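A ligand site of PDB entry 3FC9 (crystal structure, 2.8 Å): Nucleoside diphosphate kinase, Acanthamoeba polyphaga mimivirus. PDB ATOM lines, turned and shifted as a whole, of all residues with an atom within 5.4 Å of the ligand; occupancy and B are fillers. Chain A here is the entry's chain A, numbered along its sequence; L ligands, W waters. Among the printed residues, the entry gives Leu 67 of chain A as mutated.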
ATOM      1  N   LYS A  14       3.602  -5.358  -3.049  1.00  0.00           N
ATOM      2  CA  LYS A  14       2.379  -4.807  -2.473  1.00  0.00           C
ATOM      3  C   LYS A  14       1.338  -4.362  -3.498  1.00  0.00           C
ATOM      4  O   LYS A  14       1.672  -4.062  -4.648  1.00  0.00           O
ATOM      5  CB  LYS A  14       2.739  -3.662  -1.523  1.00  0.00           C
ATOM      6  CG  LYS A  14       3.497  -4.113  -0.286  1.00  0.00           C
ATOM      7  CD  LYS A  14       3.942  -2.912   0.500  1.00  0.00           C
ATOM      8  CE  LYS A  14       4.274  -3.266   1.920  1.00  0.00           C
ATOM      9  NZ  LYS A  14       4.872  -2.091   2.594  1.00  0.00           N
ATOM     10  N   TYR A  55       2.776  -8.637  10.289  1.00  0.00           N
ATOM     11  CA  TYR A  55       3.054  -7.309  10.823  1.00  0.00           C
ATOM     12  C   TYR A  55       2.783  -7.206  12.326  1.00  0.00           C
ATOM     13  O   TYR A  55       2.530  -6.117  12.834  1.00  0.00           O
ATOM     14  CB  TYR A  55       2.234  -6.263  10.072  1.00  0.00           C
ATOM     15  CG  TYR A  55       2.878  -5.725   8.812  1.00  0.00           C
ATOM     16  CD1 TYR A  55       2.152  -5.554   7.645  1.00  0.00           C
ATOM     17  CD2 TYR A  55       4.223  -5.379   8.806  1.00  0.00           C
ATOM     18  CE1 TYR A  55       2.751  -5.057   6.497  1.00  0.00           C
ATOM     19  CE2 TYR A  55       4.822  -4.882   7.658  1.00  0.00           C
ATOM     20  CZ  TYR A  55       4.083  -4.716   6.508  1.00  0.00           C
ATOM     21  OH  TYR A  55       4.709  -4.213   5.378  1.00  0.00           O
ATOM     22  N   HIS A  58       3.875  -4.655  14.767  1.00  0.00           N
ATOM     23  CA  HIS A  58       3.336  -3.320  14.533  1.00  0.00           C
ATOM     24  C   HIS A  58       1.910  -3.179  15.059  1.00  0.00           C
ATOM     25  O   HIS A  58       1.295  -2.124  14.905  1.00  0.00           O
ATOM     26  CB  HIS A  58       3.339  -2.972  13.030  1.00  0.00           C
ATOM     27  CG  HIS A  58       4.689  -2.999  12.379  1.00  0.00           C
ATOM     28  ND1 HIS A  58       5.301  -1.855  11.894  1.00  0.00           N
ATOM     29  CD2 HIS A  58       5.537  -4.025  12.111  1.00  0.00           C
ATOM     30  CE1 HIS A  58       6.473  -2.175  11.368  1.00  0.00           C
ATOM     31  NE2 HIS A  58       6.639  -3.485  11.488  1.00  0.00           N
ATOM     32  N   TYR A  63      -1.031   3.277  12.694  1.00  0.00           N
ATOM     33  CA  TYR A  63      -1.229   2.951  11.286  1.00  0.00           C
ATOM     34  C   TYR A  63      -1.599   1.486  11.017  1.00  0.00           C
ATOM     35  O   TYR A  63      -1.928   1.130   9.884  1.00  0.00           O
ATOM     36  CB  TYR A  63       0.025   3.317  10.476  1.00  0.00           C
ATOM     37  CG  TYR A  63       1.292   2.628  10.940  1.00  0.00           C
ATOM     38  CD1 TYR A  63       1.481   1.269  10.703  1.00  0.00           C
ATOM     39  CD2 TYR A  63       2.283   3.325  11.606  1.00  0.00           C
ATOM     40  CE1 TYR A  63       2.624   0.633  11.122  1.00  0.00           C
ATOM     41  CE2 TYR A  63       3.432   2.694  12.037  1.00  0.00           C
ATOM     42  CZ  TYR A  63       3.602   1.348  11.795  1.00  0.00           C
ATOM     43  OH  TYR A  63       4.745   0.699  12.203  1.00  0.00           O
ATOM     44  N   LEU A  67      -2.938   0.059   7.528  1.00  0.00           N
ATOM     45  CA  LEU A  67      -1.913  -0.773   6.916  1.00  0.00           C
ATOM     46  C   LEU A  67      -2.512  -2.090   6.449  1.00  0.00           C
ATOM     47  O   LEU A  67      -2.343  -2.482   5.299  1.00  0.00           O
ATOM     48  CB  LEU A  67      -0.785  -1.040   7.904  1.00  0.00           C
ATOM     49  CG  LEU A  67       0.266  -2.054   7.443  1.00  0.00           C
ATOM     50  CD1 LEU A  67       1.036  -1.506   6.260  1.00  0.00           C
ATOM     51  CD2 LEU A  67       1.200  -2.427   8.574  1.00  0.00           C
ATOM     52  N   PHE A  70      -5.022  -1.751   3.548  1.00  0.00           N
ATOM     53  CA  PHE A  70      -4.228  -1.591   2.349  1.00  0.00           C
ATOM     54  C   PHE A  70      -3.686  -2.920   1.805  1.00  0.00           C
ATOM     55  O   PHE A  70      -3.873  -3.240   0.640  1.00  0.00           O
ATOM     56  CB  PHE A  70      -3.084  -0.599   2.592  1.00  0.00           C
ATOM     57  CG  PHE A  70      -2.046  -0.600   1.522  1.00  0.00           C
ATOM     58  CD1 PHE A  70      -0.748  -1.016   1.789  1.00  0.00           C
ATOM     59  CD2 PHE A  70      -2.361  -0.195   0.232  1.00  0.00           C
ATOM     60  CE1 PHE A  70       0.219  -1.010   0.792  1.00  0.00           C
ATOM     61  CE2 PHE A  70      -1.403  -0.194  -0.767  1.00  0.00           C
ATOM     62  CZ  PHE A  70      -0.123  -0.606  -0.485  1.00  0.00           C
ATOM     63  N   ARG A  91      17.444  -5.022   1.362  1.00  0.00           N
ATOM     64  CA  ARG A  91      16.938  -3.875   2.101  1.00  0.00           C
ATOM     65  C   ARG A  91      17.507  -2.566   1.563  1.00  0.00           C
ATOM     66  O   ARG A  91      16.830  -1.549   1.537  1.00  0.00           O
ATOM     67  CB  ARG A  91      17.209  -3.989   3.588  1.00  0.00           C
ATOM     68  CG  ARG A  91      16.250  -4.890   4.352  1.00  0.00           C
ATOM     69  CD  ARG A  91      15.689  -4.142   5.540  1.00  0.00           C
ATOM     70  NE  ARG A  91      14.296  -3.765   5.351  1.00  0.00           N
ATOM     71  CZ  ARG A  91      13.687  -2.757   5.977  1.00  0.00           C
ATOM     72  NH1 ARG A  91      14.356  -1.986   6.834  1.00  0.00           N
ATOM     73  NH2 ARG A  91      12.400  -2.501   5.743  1.00  0.00           N
ATOM     74  N   GLN A  94      15.663  -1.827  -1.398  1.00  0.00           N
ATOM     75  CA  GLN A  94      14.332  -1.378  -0.988  1.00  0.00           C
ATOM     76  C   GLN A  94      14.300   0.143  -0.830  1.00  0.00           C
ATOM     77  O   GLN A  94      13.541   0.819  -1.515  1.00  0.00           O
ATOM     78  CB  GLN A  94      13.929  -2.069   0.317  1.00  0.00           C
ATOM     79  CG  GLN A  94      12.453  -1.944   0.674  1.00  0.00           C
ATOM     80  CD  GLN A  94      12.186  -2.150   2.156  1.00  0.00           C
ATOM     81  OE1 GLN A  94      11.296  -2.921   2.535  1.00  0.00           O
ATOM     82  NE2 GLN A  94      12.963  -1.474   2.990  1.00  0.00           N
ATOM     83  N   GLY A  95      15.147   0.670   0.054  1.00  0.00           N
ATOM     84  CA  GLY A  95      15.158   2.094   0.337  1.00  0.00           C
ATOM     85  C   GLY A  95      14.447   2.359   1.646  1.00  0.00           C
ATOM     86  O   GLY A  95      13.937   1.424   2.265  1.00  0.00           O
ATOM     87  N   ASN A  96      14.388   3.629   2.064  1.00  0.00           N
ATOM     88  CA  ASN A  96      13.797   4.010   3.344  1.00  0.00           C
ATOM     89  C   ASN A  96      12.283   4.190   3.265  1.00  0.00           C
ATOM     90  O   ASN A  96      11.761   4.722   2.282  1.00  0.00           O
ATOM     91  CB  ASN A  96      14.455   5.298   3.870  1.00  0.00           C
ATOM     92  CG  ASN A  96      14.108   5.581   5.322  1.00  0.00           C
ATOM     93  OD1 ASN A  96      13.090   6.215   5.634  1.00  0.00           O
ATOM     94  ND2 ASN A  96      14.971   5.129   6.235  1.00  0.00           N
ATOM     95  N   THR A  97      11.580   3.738   4.312  1.00  0.00           N
ATOM     96  CA  THR A  97      10.116   3.840   4.381  1.00  0.00           C
ATOM     97  C   THR A  97       9.646   5.258   4.073  1.00  0.00           C
ATOM     98  O   THR A  97       8.676   5.460   3.325  1.00  0.00           O
ATOM     99  CB  THR A  97       9.558   3.457   5.780  1.00  0.00           C
ATOM    100  OG1 THR A  97      10.288   2.358   6.329  1.00  0.00           O
ATOM    101  CG2 THR A  97       8.069   3.123   5.683  1.00  0.00           C
ATOM    102  N   ARG A 108      12.161   2.358  -3.624  1.00  0.00           N
ATOM    103  CA  ARG A 108      11.237   3.350  -3.066  1.00  0.00           C
ATOM    104  C   ARG A 108      11.607   4.772  -3.420  1.00  0.00           C
ATOM    105  O   ARG A 108      10.739   5.630  -3.542  1.00  0.00           O
ATOM    106  CB  ARG A 108      11.144   3.195  -1.546  1.00  0.00           C
ATOM    107  CG  ARG A 108      10.265   2.045  -1.072  1.00  0.00           C
ATOM    108  CD  ARG A 108      10.368   1.866   0.429  1.00  0.00           C
ATOM    109  NE  ARG A 108       9.593   0.738   0.911  1.00  0.00           N
ATOM    110  CZ  ARG A 108       9.702   0.214   2.122  1.00  0.00           C
ATOM    111  NH1 ARG A 108      10.567   0.723   2.980  1.00  0.00           N
ATOM    112  NH2 ARG A 108       8.942  -0.812   2.473  1.00  0.00           N
ATOM    113  N   ILE A 115       4.242   7.162   2.596  1.00  0.00           N
ATOM    114  CA  ILE A 115       4.741   6.487   3.780  1.00  0.00           C
ATOM    115  C   ILE A 115       4.151   5.065   3.906  1.00  0.00           C
ATOM    116  O   ILE A 115       4.841   4.134   4.342  1.00  0.00           O
ATOM    117  CB  ILE A 115       4.432   7.335   5.049  1.00  0.00           C
ATOM    118  CG1 ILE A 115       4.941   6.656   6.329  1.00  0.00           C
ATOM    119  CG2 ILE A 115       2.943   7.709   5.124  1.00  0.00           C
ATOM    120  CD1 ILE A 115       6.424   6.914   6.641  1.00  0.00           C
ATOM    121  N   ARG A 116       2.889   4.909   3.490  1.00  0.00           N
ATOM    122  CA  ARG A 116       2.173   3.642   3.582  1.00  0.00           C
ATOM    123  C   ARG A 116       2.285   2.783   2.320  1.00  0.00           C
ATOM    124  O   ARG A 116       2.712   1.627   2.379  1.00  0.00           O
ATOM    125  CB  ARG A 116       0.699   3.888   3.899  1.00  0.00           C
ATOM    126  CG  ARG A 116      -0.210   2.650   3.782  1.00  0.00           C
ATOM    127  CD  ARG A 116      -1.591   2.882   4.384  1.00  0.00           C
ATOM    128  NE  ARG A 116      -1.487   3.271   5.786  1.00  0.00           N
ATOM    129  CZ  ARG A 116      -1.937   4.415   6.291  1.00  0.00           C
ATOM    130  NH1 ARG A 116      -2.556   5.289   5.512  1.00  0.00           N
ATOM    131  NH2 ARG A 116      -1.774   4.672   7.584  1.00  0.00           N
ATOM    132  N   GLU A 117       1.897   3.342   1.188  1.00  0.00           N
ATOM    133  CA  GLU A 117       1.952   2.601  -0.069  1.00  0.00           C
ATOM    134  C   GLU A 117       3.330   2.727  -0.711  1.00  0.00           C
ATOM    135  O   GLU A 117       3.558   3.569  -1.576  1.00  0.00           O
ATOM    136  CB  GLU A 117       0.848   3.058  -1.018  1.00  0.00           C
ATOM    137  CG  GLU A 117      -0.542   2.829  -0.422  1.00  0.00           C
ATOM    138  CD  GLU A 117      -1.663   3.406  -1.261  1.00  0.00           C
ATOM    139  OE1 GLU A 117      -2.830   3.270  -0.840  1.00  0.00           O
ATOM    140  OE2 GLU A 117      -1.389   3.994  -2.322  1.00  0.00           O
ATOM    141  N   ASN A 118       4.258   1.881  -0.240  1.00  0.00           N
ATOM    142  CA  ASN A 118       5.632   1.927  -0.707  1.00  0.00           C
ATOM    143  C   ASN A 118       6.089   0.670  -1.470  1.00  0.00           C
ATOM    144  O   ASN A 118       7.258   0.276  -1.375  1.00  0.00           O
ATOM    145  CB  ASN A 118       6.581   2.248   0.443  1.00  0.00           C
ATOM    146  CG  ASN A 118       6.325   1.397   1.674  1.00  0.00           C
ATOM    147  OD1 ASN A 118       5.903   0.249   1.579  1.00  0.00           O
ATOM    148  ND2 ASN A 118       6.619   1.945   2.840  1.00  0.00           N
ATOM    149  N   ILE A 120       6.915  -2.348  -1.800  1.00  0.00           N
ATOM    150  CA  ILE A 120       7.654  -3.572  -1.447  1.00  0.00           C
ATOM    151  C   ILE A 120       7.885  -3.715   0.070  1.00  0.00           C
ATOM    152  O   ILE A 120       8.058  -2.726   0.780  1.00  0.00           O
ATOM    153  CB  ILE A 120       9.031  -3.622  -2.194  1.00  0.00           C
ATOM    154  CG1 ILE A 120       9.776  -4.922  -1.922  1.00  0.00           C
ATOM    155  CG2 ILE A 120       9.898  -2.438  -1.819  1.00  0.00           C
ATOM    156  CD1 ILE A 120      11.126  -5.012  -2.615  1.00  0.00           C
ATOM    157  N   HIS A 121       7.871  -4.953   0.556  1.00  0.00           N
ATOM    158  CA  HIS A 121       8.347  -5.253   1.902  1.00  0.00           C
ATOM    159  C   HIS A 121       9.554  -6.161   1.849  1.00  0.00           C
ATOM    160  O   HIS A 121       9.581  -7.112   1.071  1.00  0.00           O
ATOM    161  CB  HIS A 121       7.280  -5.961   2.741  1.00  0.00           C
ATOM    162  CG  HIS A 121       7.861  -6.710   3.906  1.00  0.00           C
ATOM    163  ND1 HIS A 121       7.882  -6.199   5.192  1.00  0.00           N
ATOM    164  CD2 HIS A 121       8.481  -7.913   3.966  1.00  0.00           C
ATOM    165  CE1 HIS A 121       8.482  -7.069   5.987  1.00  0.00           C
ATOM    166  NE2 HIS A 121       8.852  -8.113   5.273  1.00  0.00           N
ATOM    167  N   ALA A 122      10.551  -5.902   2.700  1.00  0.00           N
ATOM    168  CA  ALA A 122      11.723  -6.779   2.752  1.00  0.00           C
ATOM    169  C   ALA A 122      12.217  -7.025   4.176  1.00  0.00           C
ATOM    170  O   ALA A 122      12.451  -6.078   4.922  1.00  0.00           O
ATOM    171  CB  ALA A 122      12.849  -6.203   1.887  1.00  0.00           C
ATOM    172  N   SER A 123      12.367  -8.298   4.531  1.00  0.00           N
ATOM    173  CA  SER A 123      12.915  -8.666   5.844  1.00  0.00           C
ATOM    174  C   SER A 123      14.183  -7.862   6.152  1.00  0.00           C
ATOM    175  O   SER A 123      15.007  -7.597   5.263  1.00  0.00           O
ATOM    176  CB  SER A 123      13.248 -10.157   5.906  1.00  0.00           C
ATOM    177  OG  SER A 123      12.103 -10.935   5.653  1.00  0.00           O
ATOM    178  N   ASP A 124      14.322  -7.494   7.429  1.00  0.00           N
ATOM    179  CA  ASP A 124      15.413  -6.628   7.865  1.00  0.00           C
ATOM    180  C   ASP A 124      16.372  -7.282   8.845  1.00  0.00           C
ATOM    181  O   ASP A 124      17.152  -6.598   9.483  1.00  0.00           O
ATOM    182  CB  ASP A 124      14.868  -5.335   8.490  1.00  0.00           C
ATOM    183  CG  ASP A 124      14.057  -5.598   9.746  1.00  0.00           C
ATOM    184  OD1 ASP A 124      13.902  -6.789  10.131  1.00  0.00           O
ATOM    185  OD2 ASP A 124      13.562  -4.603  10.331  1.00  0.00           O
HETATM  186  N1  LIG L   1       3.405   2.180   7.353  1.00  0.00           N
HETATM  187  C1  LIG L   1       2.125   2.727   7.300  1.00  0.00           C
HETATM  188  N2  LIG L   1       1.860   3.963   7.848  1.00  0.00           N
HETATM  189  C2  LIG L   1       2.863   4.625   8.538  1.00  0.00           C
HETATM  190  C3  LIG L   1       4.132   4.047   8.649  1.00  0.00           C
HETATM  191  C4  LIG L   1       4.414   2.878   7.952  1.00  0.00           C
HETATM  192  O1  LIG L   1       1.218   2.092   6.762  1.00  0.00           O
HETATM  193  N3  LIG L   1       2.604   5.808   9.086  1.00  0.00           N
HETATM  194  C5  LIG L   1       3.632   0.839   6.774  1.00  0.00           C
HETATM  195  C6  LIG L   1       4.539   0.932   5.564  1.00  0.00           C
HETATM  196  O2  LIG L   1       3.853   0.316   4.496  1.00  0.00           O
HETATM  197  C7  LIG L   1       5.758   0.111   5.920  1.00  0.00           C
HETATM  198  C8  LIG L   1       5.222  -0.819   6.999  1.00  0.00           C
HETATM  199  O3  LIG L   1       4.264  -0.042   7.692  1.00  0.00           O
HETATM  200  O4  LIG L   1       6.289  -0.616   4.838  1.00  0.00           O
HETATM  201  C9  LIG L   1       6.322  -1.329   7.905  1.00  0.00           C
HETATM  202  O5  LIG L   1       6.728  -0.309   8.773  1.00  0.00           O
HETATM  203  P1  LIG L   1       8.246   0.213   8.724  1.00  0.00           P
HETATM  204  O6  LIG L   1       9.021  -0.789   9.546  1.00  0.00           O
HETATM  205  O7  LIG L   1       8.352   1.629   9.230  1.00  0.00           O
HETATM  206  O8  LIG L   1       8.643   0.169   7.162  1.00  0.00           O
HETATM  207  P2  LIG L   1       9.681  -0.868   6.500  1.00  0.00           P
HETATM  208  O9  LIG L   1      10.558  -0.056   5.578  1.00  0.00           O
HETATM  209  O10 LIG L   1       8.956  -1.923   5.698  1.00  0.00           O
HETATM  210  O11 LIG L   1      10.624  -1.491   7.684  1.00  0.00           O
HETATM  211  P3  LIG L   1      10.443  -2.869   8.537  1.00  0.00           P
HETATM  212  O12 LIG L   1      11.698  -3.709   8.384  1.00  0.00           O
HETATM  213  O13 LIG L   1       9.231  -3.703   8.130  1.00  0.00           O
HETATM  214  O14 LIG L   1      10.322  -2.497  10.012  1.00  0.00           O
HETATM  215  O   HOH W   1      11.224  -6.953   8.498  1.00  0.00           O
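O9 of the ligand sits at hydrogen-bond distance from OG1 of Thr 97.
The guanidinium group (NH1) of Arg 108 lies within salt-bridge range of an oxygen (O9) of the ligand, 2.7 Å away.
The backbone carbonyl oxygen (O) of Arg 116 lies within hydrogen-bond range of an oxygen (O2) of the ligand (2.7 Å).
O1 of the ligand is in hydrogen-bond range of NE of Arg 116 (3.1 Å).
An oxygen (O12) of the ligand lies within salt-bridge range of the guanidinium group (NH2) of Arg 91.
The side-chain carboxylate (OD2) of Asp 124 lies close to an oxygen (O12) of the ligand.
O4 of the ligand sits at hydrogen-bond distance from NZ of Lys 14 (3.0 Å).
ND2 of Asn 118 is in hydrogen-bond range of O4 of the ligand (3.3 Å).
The guanidinium group of Arg 108 sits at hydrogen-bond distance from the backbone carbonyl oxygen of Asn 118, at 3.3 Å.
The backbone NH of Arg 108 sits at hydrogen-bond distance from the backbone carbonyl oxygen of Gln 94 (3.0 Å).
NH2 of Arg 91 sits close to NE2 of Gln 94 (3.0 Å).
The guanidinium group of Arg 91 sits at hydrogen-bond distance from the backbone carbonyl oxygen of Ala 122, 3.0 Å away.
OD1 of Asn 118 sits at hydrogen-bond distance from NZ of Lys 14.
A ring nitrogen (ND1) of His 58 lies within hydrogen-bond range of the side-chain hydroxyl (OH) of Tyr 63 (2.6 Å).
ND2 of Asn 118 lies within hydrogen-bond range of O of Ile 115 (3.2 Å).
The side-chain amide oxygen (OE1) of Gln 94 sits at hydrogen-bond distance from the backbone NH (N) of Ala 122, at 3.1 Å.
OH of Tyr 55 touches C8 of the ligand (3.8 Å).
His 58 touches the ligand (CE1 to O5, 3.2 Å).
CB of Tyr 63 touches N2 of the ligand (3.3 Å).
Leu 67 touches the ligand (CD1 to C5, 3.5 Å).
Gln 94 touches the ligand.
Ile 115 touches the ligand (O to C6, 3.4 Å).
Hydrophobic or aromatic side chains that line the ligand: Tyr 55, His 58, Tyr 63, Leu 67 and Ile 115.
Of the 21 residues printed, 13 come within 4 Å of the ligand.
The nearest printed residue that does not touch the ligand is His 121 (4.1 Å).
Water W1 bridges OD1 of Asp 124 and O12 of the ligand.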
